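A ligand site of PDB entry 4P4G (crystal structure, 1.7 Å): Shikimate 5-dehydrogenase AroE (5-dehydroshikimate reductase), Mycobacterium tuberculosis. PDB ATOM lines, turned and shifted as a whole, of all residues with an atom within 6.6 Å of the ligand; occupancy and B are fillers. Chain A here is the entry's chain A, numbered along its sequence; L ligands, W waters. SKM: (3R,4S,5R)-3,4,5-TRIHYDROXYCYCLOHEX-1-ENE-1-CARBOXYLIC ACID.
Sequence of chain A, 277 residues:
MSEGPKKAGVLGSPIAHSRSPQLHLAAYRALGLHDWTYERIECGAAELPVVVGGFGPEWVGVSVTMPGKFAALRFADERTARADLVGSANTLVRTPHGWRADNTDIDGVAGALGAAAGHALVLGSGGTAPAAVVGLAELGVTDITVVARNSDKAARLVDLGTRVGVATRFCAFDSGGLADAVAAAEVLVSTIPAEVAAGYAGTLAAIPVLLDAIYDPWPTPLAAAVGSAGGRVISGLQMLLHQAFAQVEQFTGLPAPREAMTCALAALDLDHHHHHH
O2 of the ligand lies within hydrogen-bond range of OG of Ser 18 (2.4 Å). An oxygen (O12) of the ligand is in hydrogen-bond range of the side-chain carboxylate of Asp 105, at 2.6 Å. OG1 of Thr 65 is in hydrogen-bond range of O7 of the ligand, at 3.0 Å. O2 of the ligand is in hydrogen-bond range of OG of Ser 20 (2.7 Å). The side-chain amino group (NZ) of Lys 69 lies within hydrogen-bond range of an oxygen (O7) of the ligand (2.9 Å). The side-chain amide nitrogen of Asn 90 lies within hydrogen-bond range of an oxygen (O12) of the ligand (2.9 Å). The side-chain hydroxyl (OH) of Tyr 215 lies within hydrogen-bond range of an oxygen (O3) of the ligand. The side-chain amide oxygen (OE1) of Gln 243 lies within hydrogen-bond range of an oxygen (O11) of the ligand, 3.1 Å away. The side-chain amide nitrogen (NE2) of Gln 247 sits at hydrogen-bond distance from an oxygen (O11) of the ligand (3.0 Å).
OD1 of Asn 90 sits at hydrogen-bond distance from N of Thr 104, at 2.8 Å. The backbone carbonyl oxygen of Asn 90 sits at hydrogen-bond distance from the backbone NH of Val 64, at 2.8 Å. NZ of Lys 69 sits at hydrogen-bond distance from OG1 of Thr 128 (2.9 Å). NE2 of Gln 247 lies within hydrogen-bond range of OG1 of Thr 91 (2.9 Å). The side-chain hydroxyl (OH) of Tyr 38 sits at hydrogen-bond distance from the side-chain hydroxyl (OG) of Ser 63 (2.7 Å). The side-chain hydroxyl of Thr 104 lies within hydrogen-bond range of the backbone carbonyl oxygen of Gln 243 (2.9 Å). O of Leu 240 is in hydrogen-bond range of NE2 of Gln 243 (2.9 Å). OG of Ser 63 lies within hydrogen-bond range of OE1 of Gln 247 (2.7 Å).
Val 10 touches the ligand. CB of Ser 63 touches O11 of the ligand (3.6 Å). Val 64 touches the ligand. CD1 of Leu 240 touches C4 of the ligand, 3.8 Å away. Hydrophobic or aromatic side chains that line the ligand: Val 10, Tyr 215 and Leu 240. 13 residues have an atom within 4 Å of the ligand: Val 10, Ser 18, Ser 20, Ser 63, Val 64, Thr 65, Lys 69, Asn 90, Asp 105, Tyr 215, Leu 240, Gln 243 and Gln 247. The nearest printed residue that does not touch the ligand is His 17 (4.2 Å).
Water W1 lies within hydrogen-bond range of O3 of the ligand (2.7 Å), OG1 of Thr 65 (2.9 Å) and NE2 of His 17 (3.1 Å).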
ATOM      1  N   VAL A  10       8.938  -1.250  15.834  1.00  0.00           N
ATOM      2  CA  VAL A  10       9.201   0.180  15.854  1.00  0.00           C
ATOM      3  C   VAL A  10       8.865   0.785  14.492  1.00  0.00           C
ATOM      4  O   VAL A  10       9.204   0.212  13.444  1.00  0.00           O
ATOM      5  CB  VAL A  10      10.661   0.454  16.254  1.00  0.00           C
ATOM      6  CG1 VAL A  10      11.646  -0.219  15.309  1.00  0.00           C
ATOM      7  CG2 VAL A  10      10.917   1.966  16.344  1.00  0.00           C
ATOM      8  N   ILE A  15      14.202   4.004   9.278  1.00  0.00           N
ATOM      9  CA  ILE A  15      14.034   3.088  10.409  1.00  0.00           C
ATOM     10  C   ILE A  15      15.118   2.009  10.456  1.00  0.00           C
ATOM     11  O   ILE A  15      15.306   1.352  11.483  1.00  0.00           O
ATOM     12  CB  ILE A  15      12.617   2.452  10.401  1.00  0.00           C
ATOM     13  CG1 ILE A  15      12.289   1.841  11.769  1.00  0.00           C
ATOM     14  CG2 ILE A  15      12.509   1.402   9.292  1.00  0.00           C
ATOM     15  CD1 ILE A  15      12.239   2.866  12.892  1.00  0.00           C
ATOM     16  N   HIS A  17      18.213   1.894  10.838  1.00  0.00           N
ATOM     17  CA  HIS A  17      19.248   2.069  11.856  1.00  0.00           C
ATOM     18  C   HIS A  17      18.802   1.705  13.274  1.00  0.00           C
ATOM     19  O   HIS A  17      19.629   1.633  14.183  1.00  0.00           O
ATOM     20  CB  HIS A  17      19.634   3.545  11.914  1.00  0.00           C
ATOM     21  CG  HIS A  17      18.557   4.418  12.489  1.00  0.00           C
ATOM     22  ND1 HIS A  17      17.472   4.836  11.748  1.00  0.00           N
ATOM     23  CD2 HIS A  17      18.382   4.916  13.735  1.00  0.00           C
ATOM     24  CE1 HIS A  17      16.675   5.568  12.514  1.00  0.00           C
ATOM     25  NE2 HIS A  17      17.207   5.632  13.721  1.00  0.00           N
ATOM     26  N   SER A  18      17.493   1.516  13.490  1.00  0.00           N
ATOM     27  CA  SER A  18      16.990   1.425  14.858  1.00  0.00           C
ATOM     28  C   SER A  18      17.579   0.244  15.620  1.00  0.00           C
ATOM     29  O   SER A  18      17.607  -0.858  15.102  1.00  0.00           O
ATOM     30  CB  SER A  18      15.466   1.322  14.884  1.00  0.00           C
ATOM     31  OG  SER A  18      15.014   1.085  16.205  1.00  0.00           O
ATOM     32  N   ARG A  19      18.058   0.494  16.838  1.00  0.00           N
ATOM     33  CA  ARG A  19      18.523  -0.569  17.716  1.00  0.00           C
ATOM     34  C   ARG A  19      17.473  -0.990  18.753  1.00  0.00           C
ATOM     35  O   ARG A  19      17.784  -1.727  19.682  1.00  0.00           O
ATOM     36  CB  ARG A  19      19.831  -0.179  18.428  1.00  0.00           C
ATOM     37  CG  ARG A  19      20.973   0.261  17.526  1.00  0.00           C
ATOM     38  CD  ARG A  19      21.231  -0.711  16.400  1.00  0.00           C
ATOM     39  NE  ARG A  19      22.610  -0.627  15.898  1.00  0.00           N
ATOM     40  CZ  ARG A  19      23.063   0.312  15.064  1.00  0.00           C
ATOM     41  NH1 ARG A  19      22.262   1.274  14.619  1.00  0.00           N
ATOM     42  NH2 ARG A  19      24.328   0.279  14.679  1.00  0.00           N
ATOM     43  N   SER A  20      16.243  -0.518  18.606  1.00  0.00           N
ATOM     44  CA  SER A  20      15.154  -0.981  19.454  1.00  0.00           C
ATOM     45  C   SER A  20      14.934  -2.492  19.441  1.00  0.00           C
ATOM     46  O   SER A  20      14.693  -3.067  20.515  1.00  0.00           O
ATOM     47  CB  SER A  20      13.840  -0.267  19.127  1.00  0.00           C
ATOM     48  OG  SER A  20      13.778   0.973  19.773  1.00  0.00           O
ATOM     49  N   PRO A  21      14.960  -3.136  18.245  1.00  0.00           N
ATOM     50  CA  PRO A  21      14.698  -4.578  18.250  1.00  0.00           C
ATOM     51  C   PRO A  21      15.701  -5.344  19.102  1.00  0.00           C
ATOM     52  O   PRO A  21      15.289  -6.270  19.798  1.00  0.00           O
ATOM     53  CB  PRO A  21      14.856  -4.983  16.775  1.00  0.00           C
ATOM     54  CG  PRO A  21      14.531  -3.738  16.012  1.00  0.00           C
ATOM     55  CD  PRO A  21      15.138  -2.627  16.863  1.00  0.00           C
ATOM     56  N   HIS A  24      14.565  -4.934  22.781  1.00  0.00           N
ATOM     57  CA  HIS A  24      13.310  -5.592  23.104  1.00  0.00           C
ATOM     58  C   HIS A  24      13.427  -7.107  22.999  1.00  0.00           C
ATOM     59  O   HIS A  24      12.903  -7.834  23.848  1.00  0.00           O
ATOM     60  CB  HIS A  24      12.201  -5.096  22.181  1.00  0.00           C
ATOM     61  CG  HIS A  24      11.633  -3.784  22.586  1.00  0.00           C
ATOM     62  ND1 HIS A  24      10.393  -3.658  23.192  1.00  0.00           N
ATOM     63  CD2 HIS A  24      12.108  -2.520  22.471  1.00  0.00           C
ATOM     64  CE1 HIS A  24      10.141  -2.392  23.425  1.00  0.00           C
ATOM     65  NE2 HIS A  24      11.163  -1.680  22.984  1.00  0.00           N
ATOM     66  N   TYR A  38       9.898  -8.667  17.113  1.00  0.00           N
ATOM     67  CA  TYR A  38       9.968  -7.218  17.099  1.00  0.00           C
ATOM     68  C   TYR A  38      10.681  -6.774  15.819  1.00  0.00           C
ATOM     69  O   TYR A  38      11.863  -7.051  15.622  1.00  0.00           O
ATOM     70  CB  TYR A  38      10.710  -6.747  18.357  1.00  0.00           C
ATOM     71  CG  TYR A  38      10.652  -5.249  18.598  1.00  0.00           C
ATOM     72  CD1 TYR A  38      11.404  -4.378  17.818  1.00  0.00           C
ATOM     73  CD2 TYR A  38       9.880  -4.726  19.618  1.00  0.00           C
ATOM     74  CE1 TYR A  38      11.374  -3.012  18.037  1.00  0.00           C
ATOM     75  CE2 TYR A  38       9.848  -3.357  19.854  1.00  0.00           C
ATOM     76  CZ  TYR A  38      10.596  -2.516  19.060  1.00  0.00           C
ATOM     77  OH  TYR A  38      10.571  -1.170  19.300  1.00  0.00           O
ATOM     78  N   SER A  63       6.657   0.788  19.162  1.00  0.00           N
ATOM     79  CA  SER A  63       7.413   1.970  19.507  1.00  0.00           C
ATOM     80  C   SER A  63       7.315   2.895  18.301  1.00  0.00           C
ATOM     81  O   SER A  63       7.172   2.422  17.171  1.00  0.00           O
ATOM     82  CB  SER A  63       8.871   1.612  19.763  1.00  0.00           C
ATOM     83  OG  SER A  63       8.978   0.538  20.696  1.00  0.00           O
ATOM     84  N   VAL A  64       7.341   4.201  18.544  1.00  0.00           N
ATOM     85  CA  VAL A  64       7.212   5.158  17.441  1.00  0.00           C
ATOM     86  C   VAL A  64       8.354   6.132  17.519  1.00  0.00           C
ATOM     87  O   VAL A  64       8.601   6.734  18.570  1.00  0.00           O
ATOM     88  CB  VAL A  64       5.874   5.906  17.490  1.00  0.00           C
ATOM     89  CG1 VAL A  64       5.798   6.913  16.353  1.00  0.00           C
ATOM     90  CG2 VAL A  64       4.709   4.914  17.405  1.00  0.00           C
ATOM     91  N   THR A  65       9.093   6.259  16.427  1.00  0.00           N
ATOM     92  CA  THR A  65      10.146   7.249  16.370  1.00  0.00           C
ATOM     93  C   THR A  65       9.824   8.317  15.337  1.00  0.00           C
ATOM     94  O   THR A  65       8.695   8.376  14.807  1.00  0.00           O
ATOM     95  CB  THR A  65      11.539   6.576  16.118  1.00  0.00           C
ATOM     96  OG1 THR A  65      12.597   7.525  16.346  1.00  0.00           O
ATOM     97  CG2 THR A  65      11.634   6.037  14.694  1.00  0.00           C
ATOM     98  N   MET A  66      10.772   9.201  15.066  1.00  0.00           N
ATOM     99  CA  MET A  66      10.603  10.225  14.035  1.00  0.00           C
ATOM    100  C   MET A  66      10.204   9.605  12.696  1.00  0.00           C
ATOM    101  O   MET A  66      10.755   8.566  12.302  1.00  0.00           O
ATOM    102  CB  MET A  66      11.915  11.003  13.904  1.00  0.00           C
ATOM    103  CG  MET A  66      12.273  11.417  12.507  1.00  0.00           C
ATOM    104  SD  MET A  66      13.452  12.789  12.579  1.00  0.00           S
ATOM    105  CE  MET A  66      12.404  14.026  13.336  1.00  0.00           C
ATOM    106  N   LYS A  69       5.696  10.804  16.079  1.00  0.00           N
ATOM    107  CA  LYS A  69       5.269  10.928  17.487  1.00  0.00           C
ATOM    108  C   LYS A  69       4.016  11.783  17.729  1.00  0.00           C
ATOM    109  O   LYS A  69       3.259  11.509  18.645  1.00  0.00           O
ATOM    110  CB  LYS A  69       6.419  11.364  18.385  1.00  0.00           C
ATOM    111  CG  LYS A  69       7.577  10.356  18.351  1.00  0.00           C
ATOM    112  CD  LYS A  69       8.726  10.820  19.239  1.00  0.00           C
ATOM    113  CE  LYS A  69       9.814   9.759  19.255  1.00  0.00           C
ATOM    114  NZ  LYS A  69      10.959  10.151  20.141  1.00  0.00           N
ATOM    115  N   ASN A  90       5.689   8.202  21.968  1.00  0.00           N
ATOM    116  CA  ASN A  90       6.630   7.315  21.301  1.00  0.00           C
ATOM    117  C   ASN A  90       6.243   5.848  21.496  1.00  0.00           C
ATOM    118  O   ASN A  90       7.023   4.941  21.196  1.00  0.00           O
ATOM    119  CB  ASN A  90       8.038   7.544  21.846  1.00  0.00           C
ATOM    120  CG  ASN A  90       8.203   6.984  23.239  1.00  0.00           C
ATOM    121  OD1 ASN A  90       7.253   6.964  24.027  1.00  0.00           O
ATOM    122  ND2 ASN A  90       9.400   6.509  23.559  1.00  0.00           N
ATOM    123  N   THR A  91       5.048   5.628  22.019  1.00  0.00           N
ATOM    124  CA  THR A  91       4.602   4.277  22.365  1.00  0.00           C
ATOM    125  C   THR A  91       3.109   4.145  22.134  1.00  0.00           C
ATOM    126  O   THR A  91       2.350   5.019  22.566  1.00  0.00           O
ATOM    127  CB  THR A  91       4.881   3.974  23.863  1.00  0.00           C
ATOM    128  OG1 THR A  91       6.232   4.320  24.192  1.00  0.00           O
ATOM    129  CG2 THR A  91       4.637   2.509  24.199  1.00  0.00           C
ATOM    130  N   THR A 104       7.453   7.455  26.784  1.00  0.00           N
ATOM    131  CA  THR A 104       8.554   7.003  27.634  1.00  0.00           C
ATOM    132  C   THR A 104       9.866   7.731  27.386  1.00  0.00           C
ATOM    133  O   THR A 104      10.867   7.422  28.051  1.00  0.00           O
ATOM    134  CB  THR A 104       8.781   5.479  27.518  1.00  0.00           C
ATOM    135  OG1 THR A 104       9.353   5.189  26.236  1.00  0.00           O
ATOM    136  CG2 THR A 104       7.462   4.718  27.657  1.00  0.00           C
ATOM    137  N   ASP A 105       9.890   8.692  26.455  1.00  0.00           N
ATOM    138  CA  ASP A 105      11.107   9.498  26.210  1.00  0.00           C
ATOM    139  C   ASP A 105      11.429  10.387  27.420  1.00  0.00           C
ATOM    140  O   ASP A 105      12.570  10.819  27.584  1.00  0.00           O
ATOM    141  CB  ASP A 105      10.951  10.401  24.975  1.00  0.00           C
ATOM    142  CG  ASP A 105      11.010   9.636  23.667  1.00  0.00           C
ATOM    143  OD1 ASP A 105      11.834   8.697  23.545  1.00  0.00           O
ATOM    144  OD2 ASP A 105      10.231   9.994  22.747  1.00  0.00           O
ATOM    145  N   THR A 128      10.496  14.820  20.084  1.00  0.00           N
ATOM    146  CA  THR A 128      11.266  14.449  21.264  1.00  0.00           C
ATOM    147  C   THR A 128      11.515  15.678  22.152  1.00  0.00           C
ATOM    148  O   THR A 128      11.745  15.555  23.360  1.00  0.00           O
ATOM    149  CB  THR A 128      12.596  13.786  20.864  1.00  0.00           C
ATOM    150  OG1 THR A 128      12.334  12.665  20.012  1.00  0.00           O
ATOM    151  CG2 THR A 128      13.345  13.310  22.098  1.00  0.00           C
ATOM    152  N   ALA A 213      20.253  12.963  21.394  1.00  0.00           N
ATOM    153  CA  ALA A 213      19.257  11.933  21.070  1.00  0.00           C
ATOM    154  C   ALA A 213      19.707  11.017  19.943  1.00  0.00           C
ATOM    155  O   ALA A 213      19.233   9.884  19.814  1.00  0.00           O
ATOM    156  CB  ALA A 213      17.922  12.578  20.744  1.00  0.00           C
ATOM    157  N   TYR A 215      22.006   8.467  17.805  1.00  0.00           N
ATOM    158  CA  TYR A 215      22.965   7.406  18.102  1.00  0.00           C
ATOM    159  C   TYR A 215      23.607   6.761  16.877  1.00  0.00           C
ATOM    160  O   TYR A 215      24.520   5.959  17.015  1.00  0.00           O
ATOM    161  CB  TYR A 215      22.378   6.363  19.059  1.00  0.00           C
ATOM    162  CG  TYR A 215      21.158   5.582  18.567  1.00  0.00           C
ATOM    163  CD1 TYR A 215      21.298   4.504  17.703  1.00  0.00           C
ATOM    164  CD2 TYR A 215      19.894   5.904  19.016  1.00  0.00           C
ATOM    165  CE1 TYR A 215      20.192   3.787  17.273  1.00  0.00           C
ATOM    166  CE2 TYR A 215      18.778   5.191  18.596  1.00  0.00           C
ATOM    167  CZ  TYR A 215      18.934   4.132  17.731  1.00  0.00           C
ATOM    168  OH  TYR A 215      17.831   3.423  17.313  1.00  0.00           O
ATOM    169  N   MET A 239      19.802   7.141  26.096  1.00  0.00           N
ATOM    170  CA  MET A 239      18.385   7.532  26.054  1.00  0.00           C
ATOM    171  C   MET A 239      17.521   6.381  25.551  1.00  0.00           C
ATOM    172  O   MET A 239      16.451   6.119  26.101  1.00  0.00           O
ATOM    173  CB  MET A 239      18.166   8.771  25.173  1.00  0.00           C
ATOM    174  CG  MET A 239      16.749   9.340  25.300  1.00  0.00           C
ATOM    175  SD  MET A 239      16.472  10.773  24.239  1.00  0.00           S
ATOM    176  CE  MET A 239      18.011  11.650  24.467  1.00  0.00           C
ATOM    177  N   LEU A 240      17.996   5.676  24.527  1.00  0.00           N
ATOM    178  CA  LEU A 240      17.274   4.522  23.982  1.00  0.00           C
ATOM    179  C   LEU A 240      17.015   3.440  25.035  1.00  0.00           C
ATOM    180  O   LEU A 240      15.909   2.932  25.153  1.00  0.00           O
ATOM    181  CB  LEU A 240      18.039   3.922  22.795  1.00  0.00           C
ATOM    182  CG  LEU A 240      17.345   2.716  22.162  1.00  0.00           C
ATOM    183  CD1 LEU A 240      16.125   3.190  21.361  1.00  0.00           C
ATOM    184  CD2 LEU A 240      18.332   1.955  21.278  1.00  0.00           C
ATOM    185  N   GLN A 243      14.436   4.752  27.842  1.00  0.00           N
ATOM    186  CA  GLN A 243      13.049   4.834  27.384  1.00  0.00           C
ATOM    187  C   GLN A 243      12.492   3.449  27.066  1.00  0.00           C
ATOM    188  O   GLN A 243      11.280   3.250  27.045  1.00  0.00           O
ATOM    189  CB  GLN A 243      12.909   5.772  26.164  1.00  0.00           C
ATOM    190  CG  GLN A 243      13.575   5.304  24.887  1.00  0.00           C
ATOM    191  CD  GLN A 243      12.747   4.298  24.120  1.00  0.00           C
ATOM    192  OE1 GLN A 243      11.548   4.469  23.934  1.00  0.00           O
ATOM    193  NE2 GLN A 243      13.397   3.233  23.669  1.00  0.00           N
ATOM    194  N   GLN A 247       8.693   0.829  27.920  1.00  0.00           N
ATOM    195  CA  GLN A 247       8.022   0.260  26.753  1.00  0.00           C
ATOM    196  C   GLN A 247       7.873  -1.250  26.923  1.00  0.00           C
ATOM    197  O   GLN A 247       6.797  -1.815  26.671  1.00  0.00           O
ATOM    198  CB  GLN A 247       8.792   0.584  25.477  1.00  0.00           C
ATOM    199  CG  GLN A 247       8.572   2.000  24.989  1.00  0.00           C
ATOM    200  CD  GLN A 247       9.107   2.176  23.596  1.00  0.00           C
ATOM    201  OE1 GLN A 247       9.922   1.372  23.116  1.00  0.00           O
ATOM    202  NE2 GLN A 247       8.650   3.217  22.918  1.00  0.00           N
HETATM  203  O12 SKM L   1      11.413   7.075  21.534  1.00  0.00           O
HETATM  204  C8  SKM L   1      12.321   6.159  20.925  1.00  0.00           C
HETATM  205  C6  SKM L   1      13.287   6.937  20.082  1.00  0.00           C
HETATM  206  O7  SKM L   1      12.610   7.877  19.276  1.00  0.00           O
HETATM  207  C5  SKM L   1      14.002   6.023  19.228  1.00  0.00           C
HETATM  208  C4  SKM L   1      13.689   4.763  18.961  1.00  0.00           C
HETATM  209  C1  SKM L   1      14.562   3.959  18.017  1.00  0.00           C
HETATM  210  O2  SKM L   1      14.323   2.759  17.836  1.00  0.00           O
HETATM  211  O3  SKM L   1      15.532   4.484  17.430  1.00  0.00           O
HETATM  212  C10 SKM L   1      12.451   4.043  19.599  1.00  0.00           C
HETATM  213  C9  SKM L   1      11.510   5.149  20.156  1.00  0.00           C
HETATM  214  O11 SKM L   1      10.643   4.490  21.010  1.00  0.00           O
HETATM  215  O   HOH W   1      15.307   6.685  15.956  1.00  0.00           O
